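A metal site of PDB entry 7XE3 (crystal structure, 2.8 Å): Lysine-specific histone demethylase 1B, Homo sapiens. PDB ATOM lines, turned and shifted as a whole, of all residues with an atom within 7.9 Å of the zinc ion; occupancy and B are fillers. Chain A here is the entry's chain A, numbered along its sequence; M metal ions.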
ATOM      1  N   LYS A  23      -8.960 -25.386 -29.613  1.00  0.00           N
ATOM      2  CA  LYS A  23      -8.073 -26.435 -29.160  1.00  0.00           C
ATOM      3  C   LYS A  23      -6.742 -26.396 -29.895  1.00  0.00           C
ATOM      4  O   LYS A  23      -6.638 -25.958 -31.036  1.00  0.00           O
ATOM      5  CB  LYS A  23      -8.733 -27.806 -29.345  1.00  0.00           C
ATOM      6  CG  LYS A  23     -10.142 -27.937 -28.754  1.00  0.00           C
ATOM      7  CD  LYS A  23     -10.138 -27.825 -27.230  1.00  0.00           C
ATOM      8  CE  LYS A  23      -9.642 -29.129 -26.581  1.00  0.00           C
ATOM      9  NZ  LYS A  23      -9.024 -28.923 -25.232  1.00  0.00           N
ATOM     10  N   CYS A  24      -5.707 -26.886 -29.201  1.00  0.00           N
ATOM     11  CA  CYS A  24      -4.365 -26.929 -29.754  1.00  0.00           C
ATOM     12  C   CYS A  24      -4.325 -27.753 -31.036  1.00  0.00           C
ATOM     13  O   CYS A  24      -5.162 -28.626 -31.290  1.00  0.00           O
ATOM     14  CB  CYS A  24      -3.398 -27.511 -28.724  1.00  0.00           C
ATOM     15  SG  CYS A  24      -1.724 -27.798 -29.314  1.00  0.00           S
ATOM     16  N   GLU A  25      -3.303 -27.463 -31.853  1.00  0.00           N
ATOM     17  CA  GLU A  25      -3.095 -28.171 -33.118  1.00  0.00           C
ATOM     18  C   GLU A  25      -2.738 -29.629 -32.898  1.00  0.00           C
ATOM     19  O   GLU A  25      -3.043 -30.468 -33.751  1.00  0.00           O
ATOM     20  CB  GLU A  25      -2.002 -27.479 -33.939  1.00  0.00           C
ATOM     21  CG  GLU A  25      -0.660 -27.400 -33.179  1.00  0.00           C
ATOM     22  CD  GLU A  25       0.530 -27.036 -34.058  1.00  0.00           C
ATOM     23  OE1 GLU A  25       0.439 -27.185 -35.289  1.00  0.00           O
ATOM     24  OE2 GLU A  25       1.563 -26.611 -33.501  1.00  0.00           O
ATOM     25  N   LYS A  26      -2.091 -29.946 -31.776  1.00  0.00           N
ATOM     26  CA  LYS A  26      -1.528 -31.259 -31.521  1.00  0.00           C
ATOM     27  C   LYS A  26      -2.523 -32.112 -30.748  1.00  0.00           C
ATOM     28  O   LYS A  26      -2.920 -31.744 -29.628  1.00  0.00           O
ATOM     29  CB  LYS A  26      -0.208 -31.146 -30.734  1.00  0.00           C
ATOM     30  CG  LYS A  26       0.372 -32.472 -30.233  1.00  0.00           C
ATOM     31  CD  LYS A  26       0.916 -33.304 -31.383  1.00  0.00           C
ATOM     32  CE  LYS A  26       1.153 -34.749 -30.977  1.00  0.00           C
ATOM     33  NZ  LYS A  26       0.224 -35.684 -31.676  1.00  0.00           N
ATOM     34  N   ALA A  27      -2.937 -33.231 -31.345  1.00  0.00           N
ATOM     35  CA  ALA A  27      -3.727 -34.227 -30.641  1.00  0.00           C
ATOM     36  C   ALA A  27      -3.030 -34.612 -29.344  1.00  0.00           C
ATOM     37  O   ALA A  27      -1.808 -34.745 -29.290  1.00  0.00           O
ATOM     38  CB  ALA A  27      -3.923 -35.464 -31.515  1.00  0.00           C
ATOM     39  N   GLY A  28      -3.821 -34.771 -28.290  1.00  0.00           N
ATOM     40  CA  GLY A  28      -3.304 -35.171 -27.008  1.00  0.00           C
ATOM     41  C   GLY A  28      -2.720 -34.071 -26.161  1.00  0.00           C
ATOM     42  O   GLY A  28      -2.320 -34.337 -25.021  1.00  0.00           O
ATOM     43  N   CYS A  29      -2.643 -32.838 -26.666  1.00  0.00           N
ATOM     44  CA  CYS A  29      -2.118 -31.755 -25.833  1.00  0.00           C
ATOM     45  C   CYS A  29      -2.989 -31.574 -24.600  1.00  0.00           C
ATOM     46  O   CYS A  29      -4.220 -31.624 -24.668  1.00  0.00           O
ATOM     47  CB  CYS A  29      -2.048 -30.452 -26.627  1.00  0.00           C
ATOM     48  SG  CYS A  29      -1.498 -29.081 -25.633  1.00  0.00           S
ATOM     49  N   THR A  30      -2.356 -31.360 -23.450  1.00  0.00           N
ATOM     50  CA  THR A  30      -3.095 -31.266 -22.203  1.00  0.00           C
ATOM     51  C   THR A  30      -3.654 -29.870 -21.933  1.00  0.00           C
ATOM     52  O   THR A  30      -4.420 -29.709 -20.975  1.00  0.00           O
ATOM     53  CB  THR A  30      -2.220 -31.673 -21.019  1.00  0.00           C
ATOM     54  OG1 THR A  30      -1.112 -30.781 -20.911  1.00  0.00           O
ATOM     55  CG2 THR A  30      -1.714 -33.082 -21.214  1.00  0.00           C
ATOM     56  N   ALA A  31      -3.307 -28.867 -22.745  1.00  0.00           N
ATOM     57  CA  ALA A  31      -3.865 -27.533 -22.566  1.00  0.00           C
ATOM     58  C   ALA A  31      -5.310 -27.519 -23.023  1.00  0.00           C
ATOM     59  O   ALA A  31      -5.594 -27.646 -24.221  1.00  0.00           O
ATOM     60  CB  ALA A  31      -3.053 -26.505 -23.344  1.00  0.00           C
ATOM     61  N   THR A  32      -6.237 -27.365 -22.073  1.00  0.00           N
ATOM     62  CA  THR A  32      -7.642 -27.308 -22.463  1.00  0.00           C
ATOM     63  C   THR A  32      -7.962 -25.978 -23.137  1.00  0.00           C
ATOM     64  O   THR A  32      -8.833 -25.929 -24.011  1.00  0.00           O
ATOM     65  CB  THR A  32      -8.564 -27.554 -21.259  1.00  0.00           C
ATOM     66  OG1 THR A  32      -8.097 -26.820 -20.120  1.00  0.00           O
ATOM     67  CG2 THR A  32      -8.610 -29.037 -20.924  1.00  0.00           C
ATOM     68  N   PRO A  34      -5.650 -23.091 -24.929  1.00  0.00           N
ATOM     69  CA  PRO A  34      -4.471 -22.326 -25.368  1.00  0.00           C
ATOM     70  C   PRO A  34      -4.689 -20.819 -25.226  1.00  0.00           C
ATOM     71  O   PRO A  34      -5.747 -20.293 -25.575  1.00  0.00           O
ATOM     72  CB  PRO A  34      -4.323 -22.736 -26.830  1.00  0.00           C
ATOM     73  CG  PRO A  34      -4.993 -24.060 -26.928  1.00  0.00           C
ATOM     74  CD  PRO A  34      -6.101 -24.054 -25.943  1.00  0.00           C
ATOM     75  N   TRP A  53      -3.726 -23.022 -33.607  1.00  0.00           N
ATOM     76  CA  TRP A  53      -3.078 -22.778 -32.324  1.00  0.00           C
ATOM     77  C   TRP A  53      -1.719 -23.482 -32.344  1.00  0.00           C
ATOM     78  O   TRP A  53      -1.625 -24.689 -32.115  1.00  0.00           O
ATOM     79  CB  TRP A  53      -3.952 -23.269 -31.179  1.00  0.00           C
ATOM     80  CG  TRP A  53      -4.866 -22.220 -30.640  1.00  0.00           C
ATOM     81  CD1 TRP A  53      -6.234 -22.210 -30.707  1.00  0.00           C
ATOM     82  CD2 TRP A  53      -4.495 -21.021 -29.950  1.00  0.00           C
ATOM     83  NE1 TRP A  53      -6.739 -21.080 -30.097  1.00  0.00           N
ATOM     84  CE2 TRP A  53      -5.691 -20.331 -29.626  1.00  0.00           C
ATOM     85  CE3 TRP A  53      -3.279 -20.462 -29.580  1.00  0.00           C
ATOM     86  CZ2 TRP A  53      -5.697 -19.118 -28.946  1.00  0.00           C
ATOM     87  CZ3 TRP A  53      -3.284 -19.249 -28.900  1.00  0.00           C
ATOM     88  CH2 TRP A  53      -4.487 -18.592 -28.592  1.00  0.00           C
ATOM     89  N   TYR A  54      -0.658 -22.720 -32.587  1.00  0.00           N
ATOM     90  CA  TYR A  54       0.671 -23.323 -32.708  1.00  0.00           C
ATOM     91  C   TYR A  54       1.197 -23.760 -31.349  1.00  0.00           C
ATOM     92  O   TYR A  54       1.183 -22.979 -30.385  1.00  0.00           O
ATOM     93  CB  TYR A  54       1.626 -22.332 -33.362  1.00  0.00           C
ATOM     94  CG  TYR A  54       1.283 -22.023 -34.799  1.00  0.00           C
ATOM     95  CD1 TYR A  54       0.219 -21.186 -35.125  1.00  0.00           C
ATOM     96  CD2 TYR A  54       2.022 -22.575 -35.828  1.00  0.00           C
ATOM     97  CE1 TYR A  54      -0.093 -20.915 -36.450  1.00  0.00           C
ATOM     98  CE2 TYR A  54       1.721 -22.302 -37.154  1.00  0.00           C
ATOM     99  CZ  TYR A  54       0.670 -21.485 -37.458  1.00  0.00           C
ATOM    100  OH  TYR A  54       0.380 -21.225 -38.787  1.00  0.00           O
ATOM    101  N   HIS A  55       1.699 -25.002 -31.281  1.00  0.00           N
ATOM    102  CA  HIS A  55       2.094 -25.662 -30.039  1.00  0.00           C
ATOM    103  C   HIS A  55       3.615 -25.636 -29.889  1.00  0.00           C
ATOM    104  O   HIS A  55       4.333 -26.170 -30.734  1.00  0.00           O
ATOM    105  CB  HIS A  55       1.576 -27.103 -30.037  1.00  0.00           C
ATOM    106  CG  HIS A  55       2.067 -27.935 -28.884  1.00  0.00           C
ATOM    107  ND1 HIS A  55       1.235 -28.352 -27.871  1.00  0.00           N
ATOM    108  CD2 HIS A  55       3.289 -28.433 -28.595  1.00  0.00           C
ATOM    109  CE1 HIS A  55       1.936 -29.063 -26.999  1.00  0.00           C
ATOM    110  NE2 HIS A  55       3.179 -29.128 -27.415  1.00  0.00           N
ATOM    111  N   LEU A  56       4.100 -25.062 -28.776  1.00  0.00           N
ATOM    112  CA  LEU A  56       5.496 -25.207 -28.396  1.00  0.00           C
ATOM    113  C   LEU A  56       5.686 -26.236 -27.283  1.00  0.00           C
ATOM    114  O   LEU A  56       6.537 -27.124 -27.386  1.00  0.00           O
ATOM    115  CB  LEU A  56       6.085 -23.858 -27.936  1.00  0.00           C
ATOM    116  CG  LEU A  56       6.493 -22.809 -28.977  1.00  0.00           C
ATOM    117  CD1 LEU A  56       7.180 -21.643 -28.292  1.00  0.00           C
ATOM    118  CD2 LEU A  56       7.372 -23.385 -30.073  1.00  0.00           C
ATOM    119  N   SER A  57       4.911 -26.107 -26.215  1.00  0.00           N
ATOM    120  CA  SER A  57       4.841 -27.108 -25.165  1.00  0.00           C
ATOM    121  C   SER A  57       3.378 -27.243 -24.776  1.00  0.00           C
ATOM    122  O   SER A  57       2.518 -26.512 -25.271  1.00  0.00           O
ATOM    123  CB  SER A  57       5.702 -26.740 -23.949  1.00  0.00           C
ATOM    124  OG  SER A  57       5.060 -25.783 -23.130  1.00  0.00           O
ATOM    125  N   CYS A  58       3.087 -28.165 -23.872  1.00  0.00           N
ATOM    126  CA  CYS A  58       1.739 -28.267 -23.353  1.00  0.00           C
ATOM    127  C   CYS A  58       1.280 -26.981 -22.680  1.00  0.00           C
ATOM    128  O   CYS A  58       0.076 -26.784 -22.496  1.00  0.00           O
ATOM    129  CB  CYS A  58       1.644 -29.418 -22.357  1.00  0.00           C
ATOM    130  SG  CYS A  58       1.566 -31.003 -23.164  1.00  0.00           S
ATOM    131  N   GLY A  59       2.196 -26.108 -22.301  1.00  0.00           N
ATOM    132  CA  GLY A  59       1.788 -24.951 -21.545  1.00  0.00           C
ATOM    133  C   GLY A  59       1.994 -23.675 -22.302  1.00  0.00           C
ATOM    134  O   GLY A  59       1.732 -22.585 -21.771  1.00  0.00           O
ATOM    135  N   GLU A  60       2.452 -23.782 -23.553  1.00  0.00           N
ATOM    136  CA  GLU A  60       2.894 -22.620 -24.314  1.00  0.00           C
ATOM    137  C   GLU A  60       2.389 -22.716 -25.746  1.00  0.00           C
ATOM    138  O   GLU A  60       2.769 -23.631 -26.475  1.00  0.00           O
ATOM    139  CB  GLU A  60       4.419 -22.516 -24.275  1.00  0.00           C
ATOM    140  CG  GLU A  60       4.934 -21.990 -22.942  1.00  0.00           C
ATOM    141  CD  GLU A  60       6.321 -22.488 -22.596  1.00  0.00           C
ATOM    142  OE1 GLU A  60       6.757 -23.522 -23.156  1.00  0.00           O
ATOM    143  OE2 GLU A  60       6.972 -21.845 -21.760  1.00  0.00           O
ATOM    144  N   HIS A  61       1.537 -21.759 -26.149  1.00  0.00           N
ATOM    145  CA  HIS A  61       0.991 -21.727 -27.503  1.00  0.00           C
ATOM    146  C   HIS A  61       0.942 -20.284 -27.987  1.00  0.00           C
ATOM    147  O   HIS A  61       0.908 -19.345 -27.190  1.00  0.00           O
ATOM    148  CB  HIS A  61      -0.412 -22.335 -27.573  1.00  0.00           C
ATOM    149  CG  HIS A  61      -0.506 -23.702 -26.972  1.00  0.00           C
ATOM    150  ND1 HIS A  61      -0.451 -23.923 -25.607  1.00  0.00           N
ATOM    151  CD2 HIS A  61      -0.663 -24.923 -27.534  1.00  0.00           C
ATOM    152  CE1 HIS A  61      -0.558 -25.213 -25.367  1.00  0.00           C
ATOM    153  NE2 HIS A  61      -0.685 -25.842 -26.517  1.00  0.00           N
ATOM    154  N   MET A 175       6.155 -33.984 -25.083  1.00  0.00           N
ATOM    155  CA  MET A 175       5.307 -33.070 -25.815  1.00  0.00           C
ATOM    156  C   MET A 175       5.991 -31.764 -26.153  1.00  0.00           C
ATOM    157  O   MET A 175       5.349 -30.877 -26.722  1.00  0.00           O
ATOM    158  CB  MET A 175       4.041 -32.788 -25.017  1.00  0.00           C
ATOM    159  CG  MET A 175       3.288 -34.021 -24.673  1.00  0.00           C
ATOM    160  SD  MET A 175       2.419 -34.605 -26.113  1.00  0.00           S
ATOM    161  CE  MET A 175       0.950 -33.590 -25.956  1.00  0.00           C
HETATM  162 ZN    ZN M   1      -0.646 -27.690 -27.271  1.00  0.00          ZN
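A ring nitrogen (NE2) of His 55 sits close to the backbone carbonyl oxygen of Ser 57 (3.4 Å). The side-chain carboxylate of Glu 25 sits at hydrogen-bond distance from the backbone NH of His 55, at 2.7 Å. NE2 of His 55 sits at hydrogen-bond distance from O of Met 175 (2.9 Å). The side-chain sulfur (SG) of Cys 29 lies close to the backbone NH (N) of Ala 31 (3.4 Å). N of Lys 26 sits close to SG of Cys 24 (3.3 Å). OG of Ser 57 is in hydrogen-bond range of OE1 of Glu 60 (2.8 Å). The side-chain hydroxyl (OG) of Ser 57 lies close to the backbone NH (N) of Gly 59 (3.0 Å).
Residues that only touch the zinc ion: Ser 57 (3.9 Å). Within 4 Å of the zinc ion: Cys 24, Cys 29, His 55, Ser 57 and His 61.
NE2 of His 61 is bound to the zinc ion (2.0 Å). A ring nitrogen (ND1) of His 55 is bound to the zinc ion, at 2.1 Å. The zinc ion is bound by SG of Cys 29 (2.3 Å). The zinc ion is bound by SG of Cys 24 (2.3 Å). The zinc ion has four donor atoms within binding distance.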
